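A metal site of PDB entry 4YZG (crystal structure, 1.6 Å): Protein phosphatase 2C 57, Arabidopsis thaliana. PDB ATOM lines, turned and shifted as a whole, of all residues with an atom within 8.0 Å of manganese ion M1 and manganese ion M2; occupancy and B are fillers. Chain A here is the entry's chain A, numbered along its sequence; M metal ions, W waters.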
ATOM      1  N   ARG A  12      20.994   2.666  -0.315  1.00  0.00           N
ATOM      2  CA  ARG A  12      20.999   3.563   0.839  1.00  0.00           C
ATOM      3  C   ARG A  12      21.165   2.761   2.105  1.00  0.00           C
ATOM      4  O   ARG A  12      20.722   1.622   2.187  1.00  0.00           O
ATOM      5  CB  ARG A  12      19.681   4.344   0.938  1.00  0.00           C
ATOM      6  CG  ARG A  12      19.542   5.427  -0.073  1.00  0.00           C
ATOM      7  CD  ARG A  12      20.515   6.565   0.229  1.00  0.00           C
ATOM      8  NE  ARG A  12      20.442   7.614  -0.785  1.00  0.00           N
ATOM      9  CZ  ARG A  12      19.707   8.721  -0.667  1.00  0.00           C
ATOM     10  NH1 ARG A  12      18.969   8.938   0.404  1.00  0.00           N
ATOM     11  NH2 ARG A  12      19.721   9.620  -1.642  1.00  0.00           N
ATOM     12  N   GLU A  14      19.704   3.311   4.839  1.00  0.00           N
ATOM     13  CA  GLU A  14      18.451   3.287   5.562  1.00  0.00           C
ATOM     14  C   GLU A  14      17.305   3.363   4.572  1.00  0.00           C
ATOM     15  O   GLU A  14      17.499   3.785   3.426  1.00  0.00           O
ATOM     16  CB  GLU A  14      18.371   4.433   6.581  1.00  0.00           C
ATOM     17  CG  GLU A  14      18.314   5.810   5.947  1.00  0.00           C
ATOM     18  CD  GLU A  14      19.639   6.249   5.359  1.00  0.00           C
ATOM     19  OE1 GLU A  14      19.670   6.615   4.160  1.00  0.00           O
ATOM     20  OE2 GLU A  14      20.656   6.219   6.077  1.00  0.00           O
ATOM     21  N   MET A  15      16.127   2.914   5.003  1.00  0.00           N
ATOM     22  CA  MET A  15      14.919   3.004   4.201  1.00  0.00           C
ATOM     23  C   MET A  15      14.041   4.131   4.725  1.00  0.00           C
ATOM     24  O   MET A  15      13.532   4.059   5.845  1.00  0.00           O
ATOM     25  CB  MET A  15      14.157   1.683   4.214  1.00  0.00           C
ATOM     26  CG  MET A  15      12.866   1.694   3.373  1.00  0.00           C
ATOM     27  SD  MET A  15      13.204   2.306   1.697  1.00  0.00           S
ATOM     28  CE  MET A  15      11.739   1.731   0.858  1.00  0.00           C
ATOM     29  N   GLU A  16      13.895   5.185   3.918  1.00  0.00           N
ATOM     30  CA  GLU A  16      13.070   6.315   4.315  1.00  0.00           C
ATOM     31  C   GLU A  16      11.906   6.599   3.351  1.00  0.00           C
ATOM     32  O   GLU A  16      11.163   7.560   3.547  1.00  0.00           O
ATOM     33  CB  GLU A  16      13.925   7.567   4.542  1.00  0.00           C
ATOM     34  CG  GLU A  16      14.786   7.454   5.789  1.00  0.00           C
ATOM     35  CD  GLU A  16      15.763   8.604   5.973  1.00  0.00           C
ATOM     36  OE1 GLU A  16      15.978   9.377   5.019  1.00  0.00           O
ATOM     37  OE2 GLU A  16      16.331   8.732   7.073  1.00  0.00           O
ATOM     38  N   ASP A  17      11.722   5.741   2.347  1.00  0.00           N
ATOM     39  CA  ASP A  17      10.524   5.795   1.521  1.00  0.00           C
ATOM     40  C   ASP A  17       9.438   4.955   2.174  1.00  0.00           C
ATOM     41  O   ASP A  17       9.734   3.989   2.902  1.00  0.00           O
ATOM     42  CB  ASP A  17      10.754   5.136   0.142  1.00  0.00           C
ATOM     43  CG  ASP A  17      11.348   6.060  -0.931  1.00  0.00           C
ATOM     44  OD1 ASP A  17      11.826   7.180  -0.671  1.00  0.00           O
ATOM     45  OD2 ASP A  17      11.355   5.582  -2.111  1.00  0.00           O
ATOM     46  N   ASP A  18       8.184   5.272   1.875  1.00  0.00           N
ATOM     47  CA  ASP A  18       7.110   4.332   2.169  1.00  0.00           C
ATOM     48  C   ASP A  18       5.977   4.541   1.184  1.00  0.00           C
ATOM     49  O   ASP A  18       5.916   5.556   0.498  1.00  0.00           O
ATOM     50  CB  ASP A  18       6.616   4.472   3.629  1.00  0.00           C
ATOM     51  CG  ASP A  18       6.001   3.164   4.178  1.00  0.00           C
ATOM     52  OD1 ASP A  18       6.001   2.122   3.479  1.00  0.00           O
ATOM     53  OD2 ASP A  18       5.552   3.176   5.347  1.00  0.00           O
ATOM     54  N   PHE A  35       5.656   8.305  -0.199  1.00  0.00           N
ATOM     55  CA  PHE A  35       6.294   9.266   0.717  1.00  0.00           C
ATOM     56  C   PHE A  35       7.789   9.077   0.600  1.00  0.00           C
ATOM     57  O   PHE A  35       8.283   7.961   0.681  1.00  0.00           O
ATOM     58  CB  PHE A  35       5.872   9.002   2.164  1.00  0.00           C
ATOM     59  CG  PHE A  35       4.405   9.203   2.418  1.00  0.00           C
ATOM     60  CD1 PHE A  35       3.862  10.479   2.373  1.00  0.00           C
ATOM     61  CD2 PHE A  35       3.576   8.113   2.663  1.00  0.00           C
ATOM     62  CE1 PHE A  35       2.490  10.670   2.582  1.00  0.00           C
ATOM     63  CE2 PHE A  35       2.202   8.288   2.871  1.00  0.00           C
ATOM     64  CZ  PHE A  35       1.672   9.567   2.835  1.00  0.00           C
ATOM     65  N   ASP A  36       8.535  10.162   0.386  1.00  0.00           N
ATOM     66  CA  ASP A  36       9.987  10.026   0.380  1.00  0.00           C
ATOM     67  C   ASP A  36      10.527  10.825   1.572  1.00  0.00           C
ATOM     68  O   ASP A  36      10.602  12.053   1.514  1.00  0.00           O
ATOM     69  CB  ASP A  36      10.540  10.584  -0.948  1.00  0.00           C
ATOM     70  CG  ASP A  36      12.036  10.500  -1.040  1.00  0.00           C
ATOM     71  OD1 ASP A  36      12.717  10.277  -0.016  1.00  0.00           O
ATOM     72  OD2 ASP A  36      12.569  10.626  -2.175  1.00  0.00           O
ATOM     73  N   GLY A  37      10.877  10.134   2.643  1.00  0.00           N
ATOM     74  CA  GLY A  37      11.358  10.802   3.844  1.00  0.00           C
ATOM     75  C   GLY A  37      12.787  11.297   3.690  1.00  0.00           C
ATOM     76  O   GLY A  37      13.561  10.768   2.896  1.00  0.00           O
ATOM     77  N   HIS A  38      13.114  12.338   4.438  1.00  0.00           N
ATOM     78  CA  HIS A  38      14.501  12.755   4.572  1.00  0.00           C
ATOM     79  C   HIS A  38      14.839  13.058   6.022  1.00  0.00           C
ATOM     80  O   HIS A  38      13.968  13.469   6.804  1.00  0.00           O
ATOM     81  CB  HIS A  38      14.825  13.961   3.665  1.00  0.00           C
ATOM     82  CG  HIS A  38      13.770  15.027   3.664  1.00  0.00           C
ATOM     83  ND1 HIS A  38      12.856  15.153   2.655  1.00  0.00           N
ATOM     84  CD2 HIS A  38      13.521  16.032   4.532  1.00  0.00           C
ATOM     85  CE1 HIS A  38      12.072  16.191   2.908  1.00  0.00           C
ATOM     86  NE2 HIS A  38      12.451  16.730   4.045  1.00  0.00           N
ATOM     87  N   ALA A  39      16.106  12.845   6.370  1.00  0.00           N
ATOM     88  CA  ALA A  39      16.624  13.137   7.711  1.00  0.00           C
ATOM     89  C   ALA A  39      15.852  12.412   8.822  1.00  0.00           C
ATOM     90  O   ALA A  39      15.602  12.942   9.901  1.00  0.00           O
ATOM     91  CB  ALA A  39      16.688  14.628   7.970  1.00  0.00           C
ATOM     92  N   GLY A  40      15.486  11.169   8.522  1.00  0.00           N
ATOM     93  CA  GLY A  40      14.839  10.313   9.500  1.00  0.00           C
ATOM     94  C   GLY A  40      13.515   9.824   8.962  1.00  0.00           C
ATOM     95  O   GLY A  40      13.068  10.220   7.881  1.00  0.00           O
ATOM     96  N   VAL A  44       7.538  10.433   7.834  1.00  0.00           N
ATOM     97  CA  VAL A  44       6.860   9.379   7.046  1.00  0.00           C
ATOM     98  C   VAL A  44       5.962   8.513   7.906  1.00  0.00           C
ATOM     99  O   VAL A  44       4.821   8.209   7.525  1.00  0.00           O
ATOM    100  CB  VAL A  44       7.860   8.503   6.304  1.00  0.00           C
ATOM    101  CG1 VAL A  44       7.158   7.394   5.531  1.00  0.00           C
ATOM    102  CG2 VAL A  44       8.625   9.345   5.356  1.00  0.00           C
ATOM    103  N   GLY A 103      11.630  15.176   7.548  1.00  0.00           N
ATOM    104  CA  GLY A 103      10.529  15.653   6.727  1.00  0.00           C
ATOM    105  C   GLY A 103      10.190  14.587   5.716  1.00  0.00           C
ATOM    106  O   GLY A 103      10.768  13.505   5.721  1.00  0.00           O
ATOM    107  N   SER A 104       9.239  14.894   4.826  1.00  0.00           N
ATOM    108  CA  SER A 104       8.885  13.947   3.792  1.00  0.00           C
ATOM    109  C   SER A 104       8.205  14.645   2.642  1.00  0.00           C
ATOM    110  O   SER A 104       7.386  15.554   2.877  1.00  0.00           O
ATOM    111  CB  SER A 104       7.946  12.861   4.355  1.00  0.00           C
ATOM    112  OG  SER A 104       7.683  11.875   3.370  1.00  0.00           O
ATOM    113  N   THR A 105       8.485  14.234   1.417  1.00  0.00           N
ATOM    114  CA  THR A 105       7.648  14.641   0.294  1.00  0.00           C
ATOM    115  C   THR A 105       6.415  13.724   0.273  1.00  0.00           C
ATOM    116  O   THR A 105       6.345  12.724   1.014  1.00  0.00           O
ATOM    117  CB  THR A 105       8.401  14.564  -1.048  1.00  0.00           C
ATOM    118  OG1 THR A 105       8.807  13.201  -1.267  1.00  0.00           O
ATOM    119  CG2 THR A 105       9.637  15.463  -1.014  1.00  0.00           C
ATOM    120  N   ASP A 123       9.331  16.072  -4.841  1.00  0.00           N
ATOM    121  CA  ASP A 123      10.008  15.673  -6.064  1.00  0.00           C
ATOM    122  C   ASP A 123       9.833  14.218  -6.394  1.00  0.00           C
ATOM    123  O   ASP A 123      10.627  13.656  -7.152  1.00  0.00           O
ATOM    124  CB  ASP A 123      11.480  16.078  -6.034  1.00  0.00           C
ATOM    125  CG  ASP A 123      12.253  15.400  -4.927  1.00  0.00           C
ATOM    126  OD1 ASP A 123      11.639  14.663  -4.119  1.00  0.00           O
ATOM    127  OD2 ASP A 123      13.483  15.616  -4.854  1.00  0.00           O
ATOM    128  N   SER A 124       8.857  13.566  -5.925  1.00  0.00           N
ATOM    129  CA  SER A 124       8.348  12.366  -6.507  1.00  0.00           C
ATOM    130  C   SER A 124       7.638  12.871  -7.776  1.00  0.00           C
ATOM    131  O   SER A 124       7.651  14.076  -8.097  1.00  0.00           O
ATOM    132  CB  SER A 124       7.502  11.583  -5.499  1.00  0.00           C
ATOM    133  OG  SER A 124       8.311  11.122  -4.399  1.00  0.00           O
ATOM    134  N   SER A 238       8.968   7.503  -6.368  1.00  0.00           N
ATOM    135  CA  SER A 238       9.928   8.437  -5.762  1.00  0.00           C
ATOM    136  C   SER A 238      11.051   8.724  -6.762  1.00  0.00           C
ATOM    137  O   SER A 238      11.228   8.042  -7.781  1.00  0.00           O
ATOM    138  CB  SER A 238      10.492   7.897  -4.451  1.00  0.00           C
ATOM    139  OG  SER A 238      11.242   6.713  -4.661  1.00  0.00           O
ATOM    140  N   ASP A 239      11.800   9.764  -6.456  1.00  0.00           N
ATOM    141  CA  ASP A 239      12.907  10.188  -7.318  1.00  0.00           C
ATOM    142  C   ASP A 239      14.010   9.127  -7.457  1.00  0.00           C
ATOM    143  O   ASP A 239      14.874   9.256  -8.324  1.00  0.00           O
ATOM    144  CB  ASP A 239      13.458  11.540  -6.869  1.00  0.00           C
ATOM    145  CG  ASP A 239      14.077  11.500  -5.494  1.00  0.00           C
ATOM    146  OD1 ASP A 239      14.081  10.441  -4.801  1.00  0.00           O
ATOM    147  OD2 ASP A 239      14.618  12.544  -5.098  1.00  0.00           O
ATOM    148  N   GLY A 240      13.981   8.061  -6.647  1.00  0.00           N
ATOM    149  CA  GLY A 240      14.966   7.002  -6.831  1.00  0.00           C
ATOM    150  C   GLY A 240      14.794   6.355  -8.192  1.00  0.00           C
ATOM    151  O   GLY A 240      15.730   5.757  -8.723  1.00  0.00           O
ATOM    152  N   LEU A 241      13.584   6.468  -8.741  1.00  0.00           N
ATOM    153  CA  LEU A 241      13.331   6.068 -10.114  1.00  0.00           C
ATOM    154  C   LEU A 241      13.651   7.217 -11.078  1.00  0.00           C
ATOM    155  O   LEU A 241      14.505   7.097 -11.953  1.00  0.00           O
ATOM    156  CB  LEU A 241      11.851   5.672 -10.296  1.00  0.00           C
ATOM    157  CG  LEU A 241      11.484   5.362 -11.764  1.00  0.00           C
ATOM    158  CD1 LEU A 241      12.302   4.199 -12.333  1.00  0.00           C
ATOM    159  CD2 LEU A 241      10.001   5.060 -11.889  1.00  0.00           C
ATOM    160  N   ASP A 243      15.218  10.010 -11.066  1.00  0.00           N
ATOM    161  CA  ASP A 243      16.568  10.599 -11.198  1.00  0.00           C
ATOM    162  C   ASP A 243      17.473   9.763 -12.110  1.00  0.00           C
ATOM    163  O   ASP A 243      18.522  10.257 -12.556  1.00  0.00           O
ATOM    164  CB  ASP A 243      17.255  10.840  -9.840  1.00  0.00           C
ATOM    165  CG  ASP A 243      16.615  11.974  -9.035  1.00  0.00           C
ATOM    166  OD1 ASP A 243      15.711  12.662  -9.547  1.00  0.00           O
ATOM    167  OD2 ASP A 243      17.021  12.162  -7.862  1.00  0.00           O
ATOM    168  N   SER A 280      20.944   3.643  -9.689  1.00  0.00           N
ATOM    169  CA  SER A 280      20.246   4.463  -8.711  1.00  0.00           C
ATOM    170  C   SER A 280      20.829   4.154  -7.342  1.00  0.00           C
ATOM    171  O   SER A 280      21.007   2.999  -6.966  1.00  0.00           O
ATOM    172  CB  SER A 280      18.743   4.192  -8.699  1.00  0.00           C
ATOM    173  OG  SER A 280      18.111   4.919  -7.658  1.00  0.00           O
ATOM    174  N   GLN A 281      21.116   5.213  -6.604  1.00  0.00           N
ATOM    175  CA  GLN A 281      21.700   5.156  -5.277  1.00  0.00           C
ATOM    176  C   GLN A 281      20.733   5.480  -4.175  1.00  0.00           C
ATOM    177  O   GLN A 281      21.121   5.637  -3.027  1.00  0.00           O
ATOM    178  CB  GLN A 281      22.810   6.209  -5.140  1.00  0.00           C
ATOM    179  CG  GLN A 281      23.925   6.012  -6.129  1.00  0.00           C
ATOM    180  CD  GLN A 281      24.742   4.806  -5.753  1.00  0.00           C
ATOM    181  OE1 GLN A 281      24.595   3.746  -6.361  1.00  0.00           O
ATOM    182  NE2 GLN A 281      25.591   4.948  -4.746  1.00  0.00           N
ATOM    183  N   ASP A 282      19.497   5.595  -4.492  1.00  0.00           N
ATOM    184  CA  ASP A 282      18.477   6.052  -3.541  1.00  0.00           C
ATOM    185  C   ASP A 282      17.480   4.954  -3.273  1.00  0.00           C
ATOM    186  O   ASP A 282      17.429   3.949  -3.984  1.00  0.00           O
ATOM    187  CB  ASP A 282      17.735   7.247  -4.158  1.00  0.00           C
ATOM    188  CG  ASP A 282      16.942   8.058  -3.159  1.00  0.00           C
ATOM    189  OD1 ASP A 282      16.967   7.788  -1.931  1.00  0.00           O
ATOM    190  OD2 ASP A 282      16.247   8.999  -3.622  1.00  0.00           O
ATOM    191  N   ASN A 283      16.657   5.126  -2.227  1.00  0.00           N
ATOM    192  CA  ASN A 283      15.481   4.292  -2.064  1.00  0.00           C
ATOM    193  C   ASN A 283      14.585   4.458  -3.297  1.00  0.00           C
ATOM    194  O   ASN A 283      14.477   5.551  -3.876  1.00  0.00           O
ATOM    195  CB  ASN A 283      14.657   4.721  -0.832  1.00  0.00           C
ATOM    196  CG  ASN A 283      15.448   4.730   0.466  1.00  0.00           C
ATOM    197  OD1 ASN A 283      15.194   5.566   1.330  1.00  0.00           O
ATOM    198  ND2 ASN A 283      16.404   3.795   0.634  1.00  0.00           N
ATOM    199  N   ILE A 284      13.937   3.368  -3.718  1.00  0.00           N
ATOM    200  CA  ILE A 284      13.078   3.398  -4.895  1.00  0.00           C
ATOM    201  C   ILE A 284      11.700   2.859  -4.564  1.00  0.00           C
ATOM    202  O   ILE A 284      11.582   1.711  -4.158  1.00  0.00           O
ATOM    203  CB  ILE A 284      13.653   2.495  -6.041  1.00  0.00           C
ATOM    204  CG1 ILE A 284      15.102   2.918  -6.414  1.00  0.00           C
ATOM    205  CG2 ILE A 284      12.699   2.541  -7.249  1.00  0.00           C
ATOM    206  CD1 ILE A 284      15.876   1.826  -7.106  1.00  0.00           C
ATOM    207  N   SER A 285      10.671   3.683  -4.763  1.00  0.00           N
ATOM    208  CA  SER A 285       9.289   3.250  -4.531  1.00  0.00           C
ATOM    209  C   SER A 285       8.443   3.560  -5.745  1.00  0.00           C
ATOM    210  O   SER A 285       8.551   4.640  -6.348  1.00  0.00           O
ATOM    211  CB  SER A 285       8.720   3.965  -3.302  1.00  0.00           C
ATOM    212  OG  SER A 285       9.498   3.643  -2.151  1.00  0.00           O
HETATM  213 MN    MN M   1      14.544   9.965  -2.809  1.00  0.00          MN
HETATM  214 MN    MN M   2      14.485   9.953   1.052  1.00  0.00          MN
HETATM  215  O   HOH W   1      13.641   7.947  -2.717  1.00  0.00           O
HETATM  216  O   HOH W   2      15.810   9.681  -0.835  1.00  0.00           O
HETATM  217  O   HOH W   3      16.104   9.424   2.306  1.00  0.00           O
HETATM  218  O   HOH W   4      15.018  12.145   0.631  1.00  0.00           O
HETATM  219  O   HOH W   5      13.837   7.917   1.061  1.00  0.00           O
HETATM  220  O   HOH W   6      15.406  11.972  -2.757  1.00  0.00           O
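The backbone NH (N) of Thr 105 sits at hydrogen-bond distance from the backbone carbonyl oxygen (O) of Asp 36 (3.0 Å). The side-chain hydroxyl (OG) of Ser 104 sits close to the backbone carbonyl oxygen (O) of Asp 36 (3.5 Å). The side-chain carboxylate (OD1) of Asp 282 is in salt-bridge range of the guanidinium group (NH1) of Arg 12 (3.3 Å). O of Glu 16 sits at hydrogen-bond distance from N of Gly 37, 2.7 Å away.
Manganese ion M1 is bound by the side-chain carboxylate (OD1) of Asp 239 (2.1 Å), the side-chain carboxylate (OD2) of Asp 282 (2.1 Å), the side-chain carboxylate (OD2) of Asp 36 (2.2 Å), water W6 (2.2 Å), water W1 (2.2 Å) and water W2 (2.4 Å). Manganese ion M1 has six donor atoms within binding distance.
Water W2 lies within hydrogen-bond range of the side-chain carboxylate of Asp 282 and the guanidinium group of Arg 12. Water W3 lies within hydrogen-bond range of OE1 of Glu 16 and NH1 of Arg 12. Water W5 bridges OD1 of Asn 283 (2.7 Å) and OD1 of Asp 17 (2.8 Å).
Two residues have an atom within 4 Å of manganese ion M2: Asp 36 and Gly 37. The nearest printed residue that does not touch manganese ion M2 is Asp 17 (4.2 Å).
The side-chain carboxylate (OD1) of Asp 36 is bound to manganese ion M2, at 2.1 Å. Manganese ion M2 is bound by water W3, at 2.1 Å. Manganese ion M2 is bound by water W5 (2.1 Å). O of Gly 37 binds manganese ion M2 (2.2 Å). Manganese ion M2 is bound by water W4 (2.3 Å). Water W2 binds manganese ion M2 (2.3 Å).
Within 4 Å of manganese ion M1: Asp 36, Asp 239 and Asp 282. The nearest printed residue that does not touch manganese ion M1 is Gly 240 (4.3 Å).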
